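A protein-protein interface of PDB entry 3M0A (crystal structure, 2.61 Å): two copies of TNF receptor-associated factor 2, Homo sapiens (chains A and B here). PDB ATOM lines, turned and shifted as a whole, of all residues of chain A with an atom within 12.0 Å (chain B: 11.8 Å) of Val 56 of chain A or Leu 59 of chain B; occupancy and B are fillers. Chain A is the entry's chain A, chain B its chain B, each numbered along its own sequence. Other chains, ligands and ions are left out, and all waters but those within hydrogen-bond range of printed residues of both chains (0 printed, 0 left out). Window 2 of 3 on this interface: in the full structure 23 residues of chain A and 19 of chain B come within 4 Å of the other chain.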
ATOM      1  N   ASP A  47       7.451  -1.954  14.186  1.00  0.00           N
ATOM      2  CA  ASP A  47       6.210  -1.812  14.983  1.00  0.00           C
ATOM      3  C   ASP A  47       5.891  -2.956  16.004  1.00  0.00           C
ATOM      4  O   ASP A  47       5.244  -2.695  17.020  1.00  0.00           O
ATOM      5  CB  ASP A  47       5.005  -1.481  14.056  1.00  0.00           C
ATOM      6  N   LYS A  48       6.337  -4.191  15.739  1.00  0.00           N
ATOM      7  CA  LYS A  48       6.198  -5.296  16.709  1.00  0.00           C
ATOM      8  C   LYS A  48       7.365  -5.322  17.739  1.00  0.00           C
ATOM      9  O   LYS A  48       7.161  -5.629  18.917  1.00  0.00           O
ATOM     10  CB  LYS A  48       5.935  -6.663  16.046  1.00  0.00           C
ATOM     11  N   ILE A  49       8.576  -4.956  17.341  1.00  0.00           N
ATOM     12  CA  ILE A  49       9.607  -4.755  18.364  1.00  0.00           C
ATOM     13  C   ILE A  49       9.432  -3.454  19.182  1.00  0.00           C
ATOM     14  O   ILE A  49       9.800  -3.438  20.336  1.00  0.00           O
ATOM     15  CB  ILE A  49      11.044  -4.881  17.809  1.00  0.00           C
ATOM     16  CG1 ILE A  49      11.358  -6.339  17.483  1.00  0.00           C
ATOM     17  CG2 ILE A  49      12.068  -4.351  18.818  1.00  0.00           C
ATOM     18  CD1 ILE A  49      12.477  -6.496  16.460  1.00  0.00           C
ATOM     19  N   GLU A  50       8.884  -2.382  18.602  1.00  0.00           N
ATOM     20  CA  GLU A  50       8.706  -1.124  19.334  1.00  0.00           C
ATOM     21  C   GLU A  50       7.650  -1.302  20.407  1.00  0.00           C
ATOM     22  O   GLU A  50       7.580  -0.527  21.358  1.00  0.00           O
ATOM     23  CB  GLU A  50       8.267   0.012  18.413  1.00  0.00           C
ATOM     24  N   ALA A  51       6.826  -2.328  20.223  1.00  0.00           N
ATOM     25  CA  ALA A  51       5.719  -2.616  21.102  1.00  0.00           C
ATOM     26  C   ALA A  51       6.178  -3.465  22.295  1.00  0.00           C
ATOM     27  O   ALA A  51       5.843  -3.182  23.449  1.00  0.00           O
ATOM     28  CB  ALA A  51       4.634  -3.327  20.332  1.00  0.00           C
ATOM     29  N   LEU A  52       6.942  -4.505  21.996  1.00  0.00           N
ATOM     30  CA  LEU A  52       7.492  -5.369  22.994  1.00  0.00           C
ATOM     31  C   LEU A  52       8.571  -4.694  23.775  1.00  0.00           C
ATOM     32  O   LEU A  52       8.682  -4.901  24.956  1.00  0.00           O
ATOM     33  CB  LEU A  52       8.058  -6.594  22.345  1.00  0.00           C
ATOM     34  CG  LEU A  52       7.008  -7.665  22.232  1.00  0.00           C
ATOM     35  CD1 LEU A  52       5.690  -7.080  21.788  1.00  0.00           C
ATOM     36  CD2 LEU A  52       7.489  -8.709  21.284  1.00  0.00           C
ATOM     37  N   SER A  53       9.393  -3.897  23.124  1.00  0.00           N
ATOM     38  CA  SER A  53      10.327  -3.057  23.841  1.00  0.00           C
ATOM     39  C   SER A  53       9.596  -2.296  24.977  1.00  0.00           C
ATOM     40  O   SER A  53      10.202  -1.943  25.998  1.00  0.00           O
ATOM     41  CB  SER A  53      10.986  -2.094  22.849  1.00  0.00           C
ATOM     42  OG  SER A  53      11.780  -1.098  23.472  1.00  0.00           O
ATOM     43  N   SER A  54       8.291  -2.074  24.794  1.00  0.00           N
ATOM     44  CA  SER A  54       7.486  -1.241  25.701  1.00  0.00           C
ATOM     45  C   SER A  54       6.829  -1.989  26.826  1.00  0.00           C
ATOM     46  O   SER A  54       6.916  -1.557  27.963  1.00  0.00           O
ATOM     47  CB  SER A  54       6.405  -0.491  24.948  1.00  0.00           C
ATOM     48  OG  SER A  54       6.921   0.746  24.542  1.00  0.00           O
ATOM     49  N   LYS A  55       6.143  -3.079  26.487  1.00  0.00           N
ATOM     50  CA  LYS A  55       5.590  -4.015  27.463  1.00  0.00           C
ATOM     51  C   LYS A  55       6.638  -4.409  28.513  1.00  0.00           C
ATOM     52  O   LYS A  55       6.366  -4.448  29.706  1.00  0.00           O
ATOM     53  CB  LYS A  55       5.019  -5.258  26.749  1.00  0.00           C
ATOM     54  CG  LYS A  55       3.706  -5.001  25.971  1.00  0.00           C
ATOM     55  CD  LYS A  55       2.917  -6.296  25.616  1.00  0.00           C
ATOM     56  CE  LYS A  55       1.379  -6.196  25.977  1.00  0.00           C
ATOM     57  NZ  LYS A  55       0.508  -5.324  25.095  1.00  0.00           N
ATOM     58  N   VAL A  56       7.847  -4.632  28.039  1.00  0.00           N
ATOM     59  CA  VAL A  56       8.936  -5.081  28.838  1.00  0.00           C
ATOM     60  C   VAL A  56       9.526  -3.988  29.712  1.00  0.00           C
ATOM     61  O   VAL A  56      10.176  -4.294  30.706  1.00  0.00           O
ATOM     62  CB  VAL A  56       9.995  -5.712  27.942  1.00  0.00           C
ATOM     63  CG1 VAL A  56      11.285  -5.906  28.668  1.00  0.00           C
ATOM     64  CG2 VAL A  56       9.495  -7.022  27.425  1.00  0.00           C
ATOM     65  N   GLN A  57       9.333  -2.718  29.353  1.00  0.00           N
ATOM     66  CA  GLN A  57       9.670  -1.620  30.303  1.00  0.00           C
ATOM     67  C   GLN A  57       8.472  -1.269  31.219  1.00  0.00           C
ATOM     68  O   GLN A  57       8.598  -0.463  32.149  1.00  0.00           O
ATOM     69  CB  GLN A  57      10.297  -0.345  29.633  1.00  0.00           C
ATOM     70  CG  GLN A  57      11.410   0.330  30.543  1.00  0.00           C
ATOM     71  CD  GLN A  57      11.656   1.837  30.325  1.00  0.00           C
ATOM     72  OE1 GLN A  57      12.067   2.268  29.248  1.00  0.00           O
ATOM     73  NE2 GLN A  57      11.451   2.628  31.383  1.00  0.00           N
ATOM     74  N   GLN A  58       7.316  -1.870  30.931  1.00  0.00           N
ATOM     75  CA  GLN A  58       6.166  -1.749  31.798  1.00  0.00           C
ATOM     76  C   GLN A  58       6.337  -2.797  32.889  1.00  0.00           C
ATOM     77  O   GLN A  58       6.175  -2.497  34.075  1.00  0.00           O
ATOM     78  CB  GLN A  58       4.844  -1.902  31.032  1.00  0.00           C
ATOM     79  CG  GLN A  58       4.454  -0.677  30.179  1.00  0.00           C
ATOM     80  CD  GLN A  58       4.491   0.638  30.950  1.00  0.00           C
ATOM     81  OE1 GLN A  58       5.372   1.472  30.733  1.00  0.00           O
ATOM     82  NE2 GLN A  58       3.538   0.822  31.861  1.00  0.00           N
ATOM     83  N   LEU A  59       6.726  -4.006  32.495  1.00  0.00           N
ATOM     84  CA  LEU A  59       7.008  -5.050  33.458  1.00  0.00           C
ATOM     85  C   LEU A  59       8.190  -4.700  34.309  1.00  0.00           C
ATOM     86  O   LEU A  59       8.194  -4.933  35.500  1.00  0.00           O
ATOM     87  CB  LEU A  59       7.285  -6.356  32.762  1.00  0.00           C
ATOM     88  CG  LEU A  59       6.188  -6.811  31.823  1.00  0.00           C
ATOM     89  CD1 LEU A  59       6.439  -8.252  31.431  1.00  0.00           C
ATOM     90  CD2 LEU A  59       4.795  -6.619  32.438  1.00  0.00           C
ATOM     91  N   GLU A  60       9.202  -4.133  33.693  1.00  0.00           N
ATOM     92  CA  GLU A  60      10.370  -3.740  34.425  1.00  0.00           C
ATOM     93  C   GLU A  60      10.026  -2.688  35.450  1.00  0.00           C
ATOM     94  O   GLU A  60      10.611  -2.685  36.518  1.00  0.00           O
ATOM     95  CB  GLU A  60      11.433  -3.213  33.473  1.00  0.00           C
ATOM     96  N   ARG A  61       9.080  -1.808  35.138  1.00  0.00           N
ATOM     97  CA  ARG A  61       8.663  -0.782  36.092  1.00  0.00           C
ATOM     98  C   ARG A  61       7.768  -1.380  37.185  1.00  0.00           C
ATOM     99  O   ARG A  61       7.870  -1.004  38.350  1.00  0.00           O
ATOM    100  CB  ARG A  61       8.000   0.417  35.398  1.00  0.00           C
ATOM    101  CG  ARG A  61       8.932   1.214  34.487  1.00  0.00           C
ATOM    102  CD  ARG A  61       9.882   2.126  35.231  1.00  0.00           C
ATOM    103  NE  ARG A  61       9.313   3.463  35.370  1.00  0.00           N
ATOM    104  CZ  ARG A  61      10.012   4.545  35.691  1.00  0.00           C
ATOM    105  NH1 ARG A  61      11.320   4.465  35.905  1.00  0.00           N
ATOM    106  NH2 ARG A  61       9.397   5.714  35.795  1.00  0.00           N
ATOM    107  N   SER A  62       6.914  -2.328  36.816  1.00  0.00           N
ATOM    108  CA  SER A  62       6.131  -3.057  37.804  1.00  0.00           C
ATOM    109  C   SER A  62       7.038  -3.652  38.868  1.00  0.00           C
ATOM    110  O   SER A  62       6.880  -3.346  40.041  1.00  0.00           O
ATOM    111  CB  SER A  62       5.315  -4.156  37.143  1.00  0.00           C
ATOM    112  OG  SER A  62       4.426  -3.606  36.195  1.00  0.00           O
ATOM    113  N   ILE A  63       7.988  -4.488  38.452  1.00  0.00           N
ATOM    114  CA  ILE A  63       9.004  -5.028  39.354  1.00  0.00           C
ATOM    115  C   ILE A  63      10.015  -3.924  39.696  1.00  0.00           C
ATOM    116  O   ILE A  63      11.196  -4.163  39.955  1.00  0.00           O
ATOM    117  CB  ILE A  63       9.732  -6.234  38.726  1.00  0.00           C
ATOM    118  CG1 ILE A  63       8.741  -7.330  38.354  1.00  0.00           C
ATOM    119  CG2 ILE A  63      10.767  -6.799  39.678  1.00  0.00           C
ATOM    120  CD1 ILE A  63       9.380  -8.494  37.619  1.00  0.00           C
ATOM    121  N   LYS B  48      17.538  -5.256  17.799  1.00  0.00           N
ATOM    122  CA  LYS B  48      16.418  -4.920  18.650  1.00  0.00           C
ATOM    123  C   LYS B  48      15.877  -6.228  19.282  1.00  0.00           C
ATOM    124  O   LYS B  48      15.741  -6.344  20.524  1.00  0.00           O
ATOM    125  CB  LYS B  48      15.351  -4.150  17.848  1.00  0.00           C
ATOM    126  N   ILE B  49      15.629  -7.213  18.410  1.00  0.00           N
ATOM    127  CA  ILE B  49      15.232  -8.570  18.802  1.00  0.00           C
ATOM    128  C   ILE B  49      16.186  -9.161  19.818  1.00  0.00           C
ATOM    129  O   ILE B  49      15.777  -9.867  20.728  1.00  0.00           O
ATOM    130  CB  ILE B  49      15.162  -9.500  17.587  1.00  0.00           C
ATOM    131  CG1 ILE B  49      13.718  -9.577  17.074  1.00  0.00           C
ATOM    132  CG2 ILE B  49      15.727 -10.909  17.920  1.00  0.00           C
ATOM    133  CD1 ILE B  49      13.570  -9.794  15.545  1.00  0.00           C
ATOM    134  N   GLU B  50      17.466  -8.867  19.665  1.00  0.00           N
ATOM    135  CA  GLU B  50      18.454  -9.505  20.520  1.00  0.00           C
ATOM    136  C   GLU B  50      18.495  -8.812  21.902  1.00  0.00           C
ATOM    137  O   GLU B  50      18.466  -9.494  22.939  1.00  0.00           O
ATOM    138  CB  GLU B  50      19.828  -9.694  19.798  1.00  0.00           C
ATOM    139  N   ALA B  51      18.491  -7.481  21.923  1.00  0.00           N
ATOM    140  CA  ALA B  51      18.442  -6.762  23.196  1.00  0.00           C
ATOM    141  C   ALA B  51      17.055  -6.859  23.888  1.00  0.00           C
ATOM    142  O   ALA B  51      16.971  -6.776  25.116  1.00  0.00           O
ATOM    143  CB  ALA B  51      18.873  -5.298  23.048  1.00  0.00           C
ATOM    144  N   LEU B  52      15.982  -7.021  23.117  1.00  0.00           N
ATOM    145  CA  LEU B  52      14.704  -7.230  23.714  1.00  0.00           C
ATOM    146  C   LEU B  52      14.650  -8.646  24.356  1.00  0.00           C
ATOM    147  O   LEU B  52      14.332  -8.816  25.554  1.00  0.00           O
ATOM    148  CB  LEU B  52      13.631  -7.042  22.673  1.00  0.00           C
ATOM    149  CG  LEU B  52      12.248  -7.331  23.213  1.00  0.00           C
ATOM    150  CD1 LEU B  52      11.750  -6.173  24.063  1.00  0.00           C
ATOM    151  CD2 LEU B  52      11.402  -7.555  22.022  1.00  0.00           C
ATOM    152  N   SER B  53      14.991  -9.655  23.570  1.00  0.00           N
ATOM    153  CA  SER B  53      15.070 -11.030  24.048  1.00  0.00           C
ATOM    154  C   SER B  53      15.923 -11.286  25.309  1.00  0.00           C
ATOM    155  O   SER B  53      15.686 -12.267  26.061  1.00  0.00           O
ATOM    156  CB  SER B  53      15.577 -11.907  22.923  1.00  0.00           C
ATOM    157  OG  SER B  53      15.792 -13.215  23.397  1.00  0.00           O
ATOM    158  N   SER B  54      16.923 -10.437  25.545  1.00  0.00           N
ATOM    159  CA  SER B  54      17.695 -10.545  26.809  1.00  0.00           C
ATOM    160  C   SER B  54      17.157  -9.739  28.068  1.00  0.00           C
ATOM    161  O   SER B  54      17.606  -9.955  29.217  1.00  0.00           O
ATOM    162  CB  SER B  54      19.176 -10.274  26.542  1.00  0.00           C
ATOM    163  OG  SER B  54      19.446  -8.911  26.763  1.00  0.00           O
ATOM    164  N   LYS B  55      16.211  -8.822  27.850  1.00  0.00           N
ATOM    165  CA  LYS B  55      15.576  -8.107  28.944  1.00  0.00           C
ATOM    166  C   LYS B  55      14.478  -9.005  29.422  1.00  0.00           C
ATOM    167  O   LYS B  55      14.193  -9.064  30.603  1.00  0.00           O
ATOM    168  CB  LYS B  55      15.015  -6.763  28.504  1.00  0.00           C
ATOM    169  CG  LYS B  55      16.076  -5.776  28.110  1.00  0.00           C
ATOM    170  CD  LYS B  55      15.504  -4.364  27.877  1.00  0.00           C
ATOM    171  CE  LYS B  55      16.647  -3.310  27.805  1.00  0.00           C
ATOM    172  NZ  LYS B  55      16.361  -2.014  28.518  1.00  0.00           N
ATOM    173  N   VAL B  56      13.885  -9.740  28.500  1.00  0.00           N
ATOM    174  CA  VAL B  56      12.997 -10.786  28.939  1.00  0.00           C
ATOM    175  C   VAL B  56      13.688 -11.903  29.771  1.00  0.00           C
ATOM    176  O   VAL B  56      13.105 -12.381  30.754  1.00  0.00           O
ATOM    177  CB  VAL B  56      12.116 -11.387  27.796  1.00  0.00           C
ATOM    178  CG1 VAL B  56      11.738 -10.316  26.809  1.00  0.00           C
ATOM    179  CG2 VAL B  56      12.779 -12.561  27.157  1.00  0.00           C
ATOM    180  N   GLN B  57      14.887 -12.325  29.380  1.00  0.00           N
ATOM    181  CA  GLN B  57      15.607 -13.311  30.140  1.00  0.00           C
ATOM    182  C   GLN B  57      15.910 -12.616  31.450  1.00  0.00           C
ATOM    183  O   GLN B  57      15.561 -13.169  32.490  1.00  0.00           O
ATOM    184  CB  GLN B  57      16.885 -13.823  29.455  1.00  0.00           C
ATOM    185  N   GLN B  58      16.463 -11.396  31.421  1.00  0.00           N
ATOM    186  CA  GLN B  58      16.697 -10.633  32.671  1.00  0.00           C
ATOM    187  C   GLN B  58      15.418 -10.632  33.601  1.00  0.00           C
ATOM    188  O   GLN B  58      15.490 -10.906  34.818  1.00  0.00           O
ATOM    189  CB  GLN B  58      17.283  -9.224  32.419  1.00  0.00           C
ATOM    190  N   LEU B  59      14.253 -10.408  33.005  1.00  0.00           N
ATOM    191  CA  LEU B  59      13.002 -10.448  33.721  1.00  0.00           C
ATOM    192  C   LEU B  59      12.591 -11.808  34.229  1.00  0.00           C
ATOM    193  O   LEU B  59      12.078 -11.901  35.350  1.00  0.00           O
ATOM    194  CB  LEU B  59      11.878  -9.944  32.853  1.00  0.00           C
ATOM    195  CG  LEU B  59      11.666  -8.446  32.870  1.00  0.00           C
ATOM    196  CD1 LEU B  59      10.820  -8.136  31.671  1.00  0.00           C
ATOM    197  CD2 LEU B  59      11.005  -7.971  34.148  1.00  0.00           C
ATOM    198  N   GLU B  60      12.746 -12.876  33.457  1.00  0.00           N
ATOM    199  CA  GLU B  60      12.155 -14.098  33.980  1.00  0.00           C
ATOM    200  C   GLU B  60      13.047 -14.817  34.969  1.00  0.00           C
ATOM    201  O   GLU B  60      12.601 -15.731  35.665  1.00  0.00           O
ATOM    202  CB  GLU B  60      11.669 -15.012  32.883  1.00  0.00           C
ATOM    203  CG  GLU B  60      12.657 -15.369  31.854  1.00  0.00           C
ATOM    204  CD  GLU B  60      11.958 -16.039  30.666  1.00  0.00           C
ATOM    205  OE1 GLU B  60      10.793 -15.640  30.350  1.00  0.00           O
ATOM    206  OE2 GLU B  60      12.558 -16.972  30.052  1.00  0.00           O
ATOM    207  N   ARG B  61      14.319 -14.416  35.002  1.00  0.00           N
ATOM    208  CA  ARG B  61      15.247 -14.824  36.062  1.00  0.00           C
ATOM    209  C   ARG B  61      14.788 -14.076  37.334  1.00  0.00           C
ATOM    210  O   ARG B  61      14.712 -14.663  38.421  1.00  0.00           O
ATOM    211  CB  ARG B  61      16.716 -14.527  35.695  1.00  0.00           C
ATOM    212  N   SER B  62      14.413 -12.805  37.170  1.00  0.00           N
ATOM    213  CA  SER B  62      13.953 -12.011  38.277  1.00  0.00           C
ATOM    214  C   SER B  62      12.697 -12.597  38.976  1.00  0.00           C
ATOM    215  O   SER B  62      12.571 -12.480  40.202  1.00  0.00           O
ATOM    216  CB  SER B  62      13.743 -10.574  37.846  1.00  0.00           C
ATOM    217  OG  SER B  62      12.928  -9.902  38.796  1.00  0.00           O
ATOM    218  N   ILE B  63      11.785 -13.215  38.214  1.00  0.00           N
ATOM    219  CA  ILE B  63      10.638 -13.967  38.781  1.00  0.00           C
ATOM    220  C   ILE B  63      10.866 -15.494  38.545  1.00  0.00           C
ATOM    221  O   ILE B  63      10.000 -16.335  38.240  1.00  0.00           O
ATOM    222  CB  ILE B  63       9.252 -13.456  38.253  1.00  0.00           C
ATOM    223  CG1 ILE B  63       8.861 -14.118  36.936  1.00  0.00           C
ATOM    224  CG2 ILE B  63       9.270 -11.945  38.036  1.00  0.00           C
ATOM    225  CD1 ILE B  63       7.430 -13.939  36.564  1.00  0.00           C
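Of the printed residues of chain B, Ile 49 of chain A touches Lys 48 (3.4 Å) and Ile 49 (3.4 Å).
Of chain B, only Leu 52 (3.4 Å) comes within 4 Å of Ser 53 of chain A.
Val 56 of chain A touches just these residues of chain B: Lys 55 and Leu 59.
Gln 57 of chain A touches none of the printed residues of chain B.
Gln 58 of chain A touches none of the printed residues of chain B.
No residue of chain B comes within 4 Å of Glu 60 of chain A.
Of the printed residues of chain A, Ile 49 of chain B touches Ile 49.
Ser 53 of chain B touches none of the printed residues of chain A.
Of chain A, only Val 56 comes within 4 Å of Lys 55 of chain B.
No residue of chain A comes within 4 Å of Gln 58 of chain B.
Leu 59 of chain B touches just these residues of chain A: Val 56 (3.8 Å) and Ile 63 (3.9 Å).
No residue of chain A comes within 4 Å of Glu 60 of chain B.
Arg 61 of chain B touches none of the printed residues of chain A.
Of chain A, only Ile 63 comes within 4 Å of Ser 62 of chain B.
Of chain A, only Ile 63 comes within 4 Å of Ile 63 of chain B.
The nearest residue of chain B that does not touch Val 56 of chain A is Val 56 of chain B (4.03 Å).
The nearest residue of chain A that does not touch Leu 59 of chain B is Leu 59 of chain A (4.1 Å).
Among the printed residues, merely in contact across the chains: Ile 49 of chain A with Lys 48 of chain B (3.4 Å), Ile 49 of chain A with Ile 49 of chain B (3.4 Å), Leu 52 of chain A with Leu 52 of chain B (3.4 Å), Ser 53 of chain A with Leu 52 of chain B (3.4 Å), Val 56 of chain A with Lys 55 of chain B (3.8 Å), Val 56 of chain A with Leu 59 of chain B (3.8 Å), Ile 63 of chain A with Leu 59 of chain B (3.9 Å), Ile 63 of chain A with Ser 62 of chain B (3.9 Å) and Ile 63 of chain A with Ile 63 of chain B (3.5 Å).
Of the 17 printed residues of chain A, 5 touch a printed residue of chain B.
Hydrophobic or aromatic side chains of chain A that line the printed part of chain B: Ile 49, Leu 52, Val 56 and Ile 63.
Among the printed residues, no Asp or Glu carboxylate lies within 4 Å of a Lys or Arg side-chain nitrogen of the other chain.
Leu 52 of chain B touches its own counterpart, Leu 52 of chain A.
Ser 53 of chain A touches Leu 52 of chain B, but with the chains exchanged Leu 52 of chain A does not touch Ser 53 of chain B (7.7 Å).
Ile 63 of chain A touches Ser 62 of chain B, but with the chains exchanged Ser 62 of chain A does not touch Ile 63 of chain B (8.6 Å).
Ile 63 of chain A touches its own counterpart, Ile 63 of chain B.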
